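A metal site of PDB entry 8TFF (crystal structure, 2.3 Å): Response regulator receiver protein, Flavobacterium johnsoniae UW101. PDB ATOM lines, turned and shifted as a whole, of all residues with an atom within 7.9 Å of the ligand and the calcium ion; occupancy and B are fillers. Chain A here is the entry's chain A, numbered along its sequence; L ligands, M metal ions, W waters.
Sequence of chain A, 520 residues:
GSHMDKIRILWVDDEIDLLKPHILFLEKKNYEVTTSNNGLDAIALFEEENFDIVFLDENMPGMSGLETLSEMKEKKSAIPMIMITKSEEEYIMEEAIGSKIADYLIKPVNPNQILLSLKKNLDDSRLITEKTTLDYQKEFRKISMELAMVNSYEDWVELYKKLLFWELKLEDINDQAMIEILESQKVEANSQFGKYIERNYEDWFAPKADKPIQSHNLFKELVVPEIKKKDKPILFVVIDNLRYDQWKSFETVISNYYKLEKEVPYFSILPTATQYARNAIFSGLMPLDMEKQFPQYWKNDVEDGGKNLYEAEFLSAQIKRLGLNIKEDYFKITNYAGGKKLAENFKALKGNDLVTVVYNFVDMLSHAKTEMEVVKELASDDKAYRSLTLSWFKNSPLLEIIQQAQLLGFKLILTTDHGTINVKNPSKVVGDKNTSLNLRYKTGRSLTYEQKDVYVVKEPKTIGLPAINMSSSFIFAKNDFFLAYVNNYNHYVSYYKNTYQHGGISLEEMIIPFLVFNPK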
ATOM      1  N   VAL A  12      33.299 -18.698  -9.716  1.00  0.00           N
ATOM      2  CA  VAL A  12      32.509 -19.681 -10.433  1.00  0.00           C
ATOM      3  C   VAL A  12      31.060 -19.194 -10.463  1.00  0.00           C
ATOM      4  O   VAL A  12      30.402 -19.036  -9.413  1.00  0.00           O
ATOM      5  CB  VAL A  12      32.597 -21.053  -9.742  1.00  0.00           C
ATOM      6  CG1 VAL A  12      32.067 -22.174 -10.657  1.00  0.00           C
ATOM      7  CG2 VAL A  12      34.000 -21.369  -9.267  1.00  0.00           C
ATOM      8  N   ASP A  13      30.554 -19.004 -11.670  1.00  0.00           N
ATOM      9  CA  ASP A  13      29.192 -18.542 -11.885  1.00  0.00           C
ATOM     10  C   ASP A  13      28.889 -18.769 -13.368  1.00  0.00           C
ATOM     11  O   ASP A  13      29.718 -18.459 -14.223  1.00  0.00           O
ATOM     12  CB  ASP A  13      29.037 -17.054 -11.537  1.00  0.00           C
ATOM     13  CG  ASP A  13      27.606 -16.577 -11.387  1.00  0.00           C
ATOM     14  OD1 ASP A  13      26.806 -16.766 -12.323  1.00  0.00           O
ATOM     15  OD2 ASP A  13      27.282 -16.031 -10.295  1.00  0.00           O
ATOM     16  N   ASP A  14      27.699 -19.267 -13.682  1.00  0.00           N
ATOM     17  CA  ASP A  14      27.319 -19.527 -15.060  1.00  0.00           C
ATOM     18  C   ASP A  14      27.053 -18.222 -15.812  1.00  0.00           C
ATOM     19  O   ASP A  14      26.895 -18.276 -17.017  1.00  0.00           O
ATOM     20  CB  ASP A  14      26.116 -20.460 -15.188  1.00  0.00           C
ATOM     21  CG  ASP A  14      24.890 -19.973 -14.436  1.00  0.00           C
ATOM     22  OD1 ASP A  14      25.048 -19.175 -13.493  1.00  0.00           O
ATOM     23  OD2 ASP A  14      23.777 -20.397 -14.784  1.00  0.00           O
ATOM     24  N   GLU A  15      27.016 -17.083 -15.116  1.00  0.00           N
ATOM     25  CA  GLU A  15      26.690 -15.802 -15.743  1.00  0.00           C
ATOM     26  C   GLU A  15      27.774 -14.786 -15.431  1.00  0.00           C
ATOM     27  O   GLU A  15      27.515 -13.740 -14.846  1.00  0.00           O
ATOM     28  CB  GLU A  15      25.337 -15.284 -15.247  1.00  0.00           C
ATOM     29  CG  GLU A  15      24.189 -16.248 -15.428  1.00  0.00           C
ATOM     30  CD  GLU A  15      22.877 -15.731 -14.858  1.00  0.00           C
ATOM     31  OE1 GLU A  15      22.847 -15.307 -13.668  1.00  0.00           O
ATOM     32  OE2 GLU A  15      21.890 -15.732 -15.616  1.00  0.00           O
ATOM     33  N   LEU A  19      28.743 -10.212 -13.919  1.00  0.00           N
ATOM     34  CA  LEU A  19      29.605  -9.895 -12.781  1.00  0.00           C
ATOM     35  C   LEU A  19      30.791  -9.029 -13.207  1.00  0.00           C
ATOM     36  O   LEU A  19      31.670  -8.746 -12.390  1.00  0.00           O
ATOM     37  CB  LEU A  19      30.155 -11.180 -12.167  1.00  0.00           C
ATOM     38  CG  LEU A  19      29.153 -12.296 -11.883  1.00  0.00           C
ATOM     39  CD1 LEU A  19      29.861 -13.490 -11.293  1.00  0.00           C
ATOM     40  CD2 LEU A  19      28.013 -11.823 -10.987  1.00  0.00           C
ATOM     41  N   ASN A  37      32.832 -20.759 -15.606  1.00  0.00           N
ATOM     42  CA  ASN A  37      31.386 -20.671 -15.756  1.00  0.00           C
ATOM     43  C   ASN A  37      30.692 -21.978 -15.391  1.00  0.00           C
ATOM     44  O   ASN A  37      29.479 -22.091 -15.560  1.00  0.00           O
ATOM     45  CB  ASN A  37      30.963 -20.199 -17.161  1.00  0.00           C
ATOM     46  CG  ASN A  37      31.490 -21.070 -18.283  1.00  0.00           C
ATOM     47  OD1 ASN A  37      31.942 -22.195 -18.058  1.00  0.00           O
ATOM     48  ND2 ASN A  37      31.428 -20.537 -19.482  1.00  0.00           N
ATOM     49  N   LEU A  56      31.565 -18.679  -5.202  1.00  0.00           N
ATOM     50  CA  LEU A  56      30.694 -19.694  -5.801  1.00  0.00           C
ATOM     51  C   LEU A  56      29.270 -19.179  -5.907  1.00  0.00           C
ATOM     52  O   LEU A  56      28.661 -18.795  -4.895  1.00  0.00           O
ATOM     53  CB  LEU A  56      30.687 -20.964  -4.928  1.00  0.00           C
ATOM     54  CG  LEU A  56      32.052 -21.622  -4.706  1.00  0.00           C
ATOM     55  CD1 LEU A  56      32.021 -22.617  -3.571  1.00  0.00           C
ATOM     56  CD2 LEU A  56      32.484 -22.316  -5.977  1.00  0.00           C
ATOM     57  N   ASP A  57      28.730 -19.217  -7.139  1.00  0.00           N
ATOM     58  CA  ASP A  57      27.291 -19.136  -7.361  1.00  0.00           C
ATOM     59  C   ASP A  57      26.666 -20.434  -6.861  1.00  0.00           C
ATOM     60  O   ASP A  57      27.353 -21.435  -6.855  1.00  0.00           O
ATOM     61  CB  ASP A  57      26.996 -18.957  -8.848  1.00  0.00           C
ATOM     62  CG  ASP A  57      25.543 -18.640  -9.161  1.00  0.00           C
ATOM     63  OD1 ASP A  57      24.808 -18.197  -8.251  1.00  0.00           O
ATOM     64  OD2 ASP A  57      25.155 -18.861 -10.321  1.00  0.00           O
ATOM     65  N   GLU A  58      25.388 -20.425  -6.472  1.00  0.00           N
ATOM     66  CA  GLU A  58      24.750 -21.647  -6.008  1.00  0.00           C
ATOM     67  C   GLU A  58      23.988 -22.347  -7.138  1.00  0.00           C
ATOM     68  O   GLU A  58      24.185 -23.528  -7.347  1.00  0.00           O
ATOM     69  CB  GLU A  58      23.806 -21.399  -4.825  1.00  0.00           C
ATOM     70  CG  GLU A  58      22.876 -22.602  -4.530  1.00  0.00           C
ATOM     71  CD  GLU A  58      23.528 -23.964  -4.248  1.00  0.00           C
ATOM     72  OE1 GLU A  58      24.776 -24.061  -4.233  1.00  0.00           O
ATOM     73  OE2 GLU A  58      22.775 -24.927  -4.009  1.00  0.00           O
ATOM     74  N   ASN A  59      23.091 -21.598  -7.796  1.00  0.00           N
ATOM     75  CA  ASN A  59      22.214 -22.137  -8.817  1.00  0.00           C
ATOM     76  C   ASN A  59      22.962 -22.141 -10.147  1.00  0.00           C
ATOM     77  O   ASN A  59      23.051 -21.108 -10.808  1.00  0.00           O
ATOM     78  CB  ASN A  59      20.936 -21.297  -8.917  1.00  0.00           C
ATOM     79  CG  ASN A  59      20.325 -20.928  -7.574  1.00  0.00           C
ATOM     80  OD1 ASN A  59      20.263 -19.759  -7.204  1.00  0.00           O
ATOM     81  ND2 ASN A  59      19.833 -21.928  -6.859  1.00  0.00           N
ATOM     82  N   MET A  60      23.517 -23.313 -10.513  1.00  0.00           N
ATOM     83  CA  MET A  60      24.160 -23.505 -11.804  1.00  0.00           C
ATOM     84  C   MET A  60      23.640 -24.800 -12.426  1.00  0.00           C
ATOM     85  O   MET A  60      23.364 -25.774 -11.722  1.00  0.00           O
ATOM     86  CB  MET A  60      25.677 -23.583 -11.631  1.00  0.00           C
ATOM     87  CG  MET A  60      26.296 -22.217 -11.344  1.00  0.00           C
ATOM     88  SD  MET A  60      28.068 -22.276 -11.244  1.00  0.00           S
ATOM     89  CE  MET A  60      28.308 -23.286  -9.774  1.00  0.00           C
ATOM     90  N   PRO A  61      23.482 -24.849 -13.774  1.00  0.00           N
ATOM     91  CA  PRO A  61      22.807 -25.965 -14.423  1.00  0.00           C
ATOM     92  C   PRO A  61      23.515 -27.285 -14.202  1.00  0.00           C
ATOM     93  O   PRO A  61      22.858 -28.308 -14.097  1.00  0.00           O
ATOM     94  CB  PRO A  61      22.720 -25.611 -15.911  1.00  0.00           C
ATOM     95  CG  PRO A  61      23.543 -24.326 -16.094  1.00  0.00           C
ATOM     96  CD  PRO A  61      23.851 -23.787 -14.726  1.00  0.00           C
ATOM     97  N   GLY A  65      26.799 -24.812  -6.637  1.00  0.00           N
ATOM     98  CA  GLY A  65      27.843 -24.188  -5.846  1.00  0.00           C
ATOM     99  C   GLY A  65      28.303 -25.068  -4.677  1.00  0.00           C
ATOM    100  O   GLY A  65      29.502 -25.233  -4.422  1.00  0.00           O
ATOM    101  N   MET A  83      30.064 -17.800  -0.890  1.00  0.00           N
ATOM    102  CA  MET A  83      28.948 -18.003  -1.774  1.00  0.00           C
ATOM    103  C   MET A  83      28.358 -16.637  -2.133  1.00  0.00           C
ATOM    104  O   MET A  83      28.054 -15.838  -1.250  1.00  0.00           O
ATOM    105  CB  MET A  83      27.912 -18.923  -1.118  1.00  0.00           C
ATOM    106  CG  MET A  83      26.623 -19.118  -1.905  1.00  0.00           C
ATOM    107  SD  MET A  83      25.993 -20.807  -1.732  1.00  0.00           S
ATOM    108  CE  MET A  83      27.277 -21.708  -2.585  1.00  0.00           C
ATOM    109  N   ILE A  84      28.193 -16.397  -3.432  1.00  0.00           N
ATOM    110  CA  ILE A  84      27.563 -15.182  -3.930  1.00  0.00           C
ATOM    111  C   ILE A  84      26.408 -15.596  -4.842  1.00  0.00           C
ATOM    112  O   ILE A  84      26.655 -16.065  -5.946  1.00  0.00           O
ATOM    113  CB  ILE A  84      28.587 -14.271  -4.642  1.00  0.00           C
ATOM    114  CG1 ILE A  84      29.771 -13.936  -3.734  1.00  0.00           C
ATOM    115  CG2 ILE A  84      27.924 -13.010  -5.134  1.00  0.00           C
ATOM    116  CD1 ILE A  84      30.852 -13.076  -4.338  1.00  0.00           C
ATOM    117  N   THR A  85      25.172 -15.395  -4.377  1.00  0.00           N
ATOM    118  CA  THR A  85      24.029 -16.076  -4.941  1.00  0.00           C
ATOM    119  C   THR A  85      22.803 -15.188  -4.818  1.00  0.00           C
ATOM    120  O   THR A  85      22.710 -14.363  -3.911  1.00  0.00           O
ATOM    121  CB  THR A  85      23.794 -17.415  -4.236  1.00  0.00           C
ATOM    122  OG1 THR A  85      22.543 -17.957  -4.656  1.00  0.00           O
ATOM    123  CG2 THR A  85      23.738 -17.290  -2.729  1.00  0.00           C
ATOM    124  N   LYS A  86      21.847 -15.385  -5.723  1.00  0.00           N
ATOM    125  CA  LYS A  86      20.570 -14.687  -5.649  1.00  0.00           C
ATOM    126  C   LYS A  86      19.643 -15.415  -4.684  1.00  0.00           C
ATOM    127  O   LYS A  86      18.654 -14.820  -4.245  1.00  0.00           O
ATOM    128  CB  LYS A  86      19.999 -14.444  -7.050  1.00  0.00           C
ATOM    129  CG  LYS A  86      19.578 -15.659  -7.880  1.00  0.00           C
ATOM    130  CD  LYS A  86      19.471 -15.351  -9.377  1.00  0.00           C
ATOM    131  CE  LYS A  86      18.499 -16.269 -10.119  1.00  0.00           C
ATOM    132  NZ  LYS A  86      18.815 -17.702  -9.899  1.00  0.00           N
ATOM    133  N   SER A  87      19.974 -16.661  -4.292  1.00  0.00           N
ATOM    134  CA  SER A  87      19.099 -17.426  -3.403  1.00  0.00           C
ATOM    135  C   SER A  87      18.983 -16.788  -2.017  1.00  0.00           C
ATOM    136  O   SER A  87      20.008 -16.620  -1.348  1.00  0.00           O
ATOM    137  CB  SER A  87      19.545 -18.865  -3.243  1.00  0.00           C
ATOM    138  OG  SER A  87      19.068 -19.676  -4.324  1.00  0.00           O
ATOM    139  N   ILE A  92      18.798 -22.971   1.886  1.00  0.00           N
ATOM    140  CA  ILE A  92      20.076 -22.823   1.194  1.00  0.00           C
ATOM    141  C   ILE A  92      21.109 -22.173   2.122  1.00  0.00           C
ATOM    142  O   ILE A  92      22.261 -22.573   2.175  1.00  0.00           O
ATOM    143  CB  ILE A  92      19.878 -22.087  -0.141  1.00  0.00           C
ATOM    144  CG1 ILE A  92      19.055 -22.986  -1.074  1.00  0.00           C
ATOM    145  CG2 ILE A  92      21.215 -21.744  -0.773  1.00  0.00           C
ATOM    146  CD1 ILE A  92      18.296 -22.263  -2.193  1.00  0.00           C
ATOM    147  N   TYR A 104      28.419 -15.648   2.850  1.00  0.00           N
ATOM    148  CA  TYR A 104      27.325 -15.835   1.919  1.00  0.00           C
ATOM    149  C   TYR A 104      26.736 -14.451   1.611  1.00  0.00           C
ATOM    150  O   TYR A 104      26.192 -13.819   2.498  1.00  0.00           O
ATOM    151  CB  TYR A 104      26.349 -16.818   2.565  1.00  0.00           C
ATOM    152  CG  TYR A 104      25.111 -17.217   1.788  1.00  0.00           C
ATOM    153  CD1 TYR A 104      24.111 -16.320   1.476  1.00  0.00           C
ATOM    154  CD2 TYR A 104      24.907 -18.536   1.427  1.00  0.00           C
ATOM    155  CE1 TYR A 104      22.960 -16.717   0.804  1.00  0.00           C
ATOM    156  CE2 TYR A 104      23.762 -18.964   0.775  1.00  0.00           C
ATOM    157  CZ  TYR A 104      22.777 -18.051   0.452  1.00  0.00           C
ATOM    158  OH  TYR A 104      21.651 -18.491  -0.200  1.00  0.00           O
ATOM    159  N   LEU A 105      26.901 -13.981   0.377  1.00  0.00           N
ATOM    160  CA  LEU A 105      26.504 -12.650  -0.062  1.00  0.00           C
ATOM    161  C   LEU A 105      25.368 -12.788  -1.073  1.00  0.00           C
ATOM    162  O   LEU A 105      25.514 -13.503  -2.072  1.00  0.00           O
ATOM    163  CB  LEU A 105      27.698 -11.944  -0.716  1.00  0.00           C
ATOM    164  CG  LEU A 105      28.967 -11.899   0.125  1.00  0.00           C
ATOM    165  CD1 LEU A 105      30.085 -11.114  -0.563  1.00  0.00           C
ATOM    166  CD2 LEU A 105      28.674 -11.325   1.518  1.00  0.00           C
ATOM    167  N   ILE A 106      24.269 -12.086  -0.804  1.00  0.00           N
ATOM    168  CA  ILE A 106      23.066 -12.192  -1.601  1.00  0.00           C
ATOM    169  C   ILE A 106      23.073 -11.137  -2.705  1.00  0.00           C
ATOM    170  O   ILE A 106      23.321  -9.956  -2.442  1.00  0.00           O
ATOM    171  CB  ILE A 106      21.845 -12.041  -0.689  1.00  0.00           C
ATOM    172  CG1 ILE A 106      21.833 -13.138   0.381  1.00  0.00           C
ATOM    173  CG2 ILE A 106      20.552 -12.001  -1.503  1.00  0.00           C
ATOM    174  CD1 ILE A 106      20.582 -13.064   1.298  1.00  0.00           C
ATOM    175  N   LYS A 107      22.822 -11.596  -3.943  1.00  0.00           N
ATOM    176  CA  LYS A 107      22.745 -10.731  -5.108  1.00  0.00           C
ATOM    177  C   LYS A 107      21.422  -9.958  -5.103  1.00  0.00           C
ATOM    178  O   LYS A 107      20.399 -10.507  -4.700  1.00  0.00           O
ATOM    179  CB  LYS A 107      22.782 -11.532  -6.412  1.00  0.00           C
ATOM    180  CG  LYS A 107      24.133 -12.029  -6.865  1.00  0.00           C
ATOM    181  CD  LYS A 107      24.016 -13.026  -7.983  1.00  0.00           C
ATOM    182  CE  LYS A 107      25.345 -13.667  -8.323  1.00  0.00           C
ATOM    183  NZ  LYS A 107      25.203 -14.749  -9.305  1.00  0.00           N
HETATM  184 BE1  LIG L   1      22.809 -17.932  -8.511  1.00  0.00          BE
HETATM  185  F1  LIG L   1      23.168 -16.234  -8.349  1.00  0.00           F
HETATM  186  F2  LIG L   1      23.015 -18.971  -7.118  1.00  0.00           F
HETATM  187  F3  LIG L   1      22.236 -18.541 -10.045  1.00  0.00           F
HETATM  188 CA    CA M   1      23.350 -18.975 -11.735  1.00  0.00          CA
HETATM  189  O   HOH W   1      21.554 -19.884 -13.232  1.00  0.00           O
HETATM  190  O   HOH W   2      24.297 -16.757 -11.933  1.00  0.00           O
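The side-chain carboxylate (OD1) of Asp 57 is bound to a beryllium atom (BE1) of the ligand. F2 of the ligand sits at hydrogen-bond distance from N of Asn 59 (2.7 Å). OD1 of Asn 59 sits close to F2 of the ligand (2.9 Å). The side-chain amino group (NZ) of Lys 107 is in hydrogen-bond range of a fluorine (F1) of the ligand (2.7 Å). OG1 of Thr 85 is in hydrogen-bond range of F2 of the ligand (2.7 Å). The backbone NH of Glu 58 sits at hydrogen-bond distance from a fluorine (F2) of the ligand (2.9 Å). F1 of the ligand is in hydrogen-bond range of N of Lys 86 (3.1 Å).
The backbone carbonyl oxygen (O) of Asp 57 sits close to the backbone NH (N) of Gly 65 (3.4 Å). The backbone NH (N) of Asp 57 is in hydrogen-bond range of the backbone carbonyl oxygen (O) of Val 12 (2.8 Å). The side-chain amide oxygen (OD1) of Asn 59 lies within hydrogen-bond range of the side-chain hydroxyl (OG) of Ser 87 (3.1 Å). O of Thr 85 is in hydrogen-bond range of N of Lys 107 (2.8 Å). NZ of Lys 107 is in salt-bridge range of OD2 of Asp 13 (2.6 Å). The side-chain hydroxyl (OG1) of Thr 85 lies within hydrogen-bond range of the backbone NH (N) of Ser 87, 2.9 Å away. O of Leu 105 sits at hydrogen-bond distance from N of Thr 85 (3.0 Å). N of Gly 65 is in hydrogen-bond range of O of Glu 58 (3.0 Å).
Three residues have an atom within 4 Å of the calcium ion: Asp 14, Asp 57 and Asn 59.
A fluorine (F3) of the ligand binds the calcium ion. The calcium ion is bound by OD2 of Asp 57 (2.3 Å). The calcium ion is bound by O of Asn 59 (2.3 Å). Water W2 is bound to the calcium ion. OD1 of Asp 14 binds the calcium ion (2.5 Å). Water W1 is bound to the calcium ion (2.5 Å).
Water W2 lies within hydrogen-bond range of OD1 of Asp 13 (2.5 Å), OE1 of Glu 15 (2.7 Å) and NZ of Lys 107 (3.4 Å).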
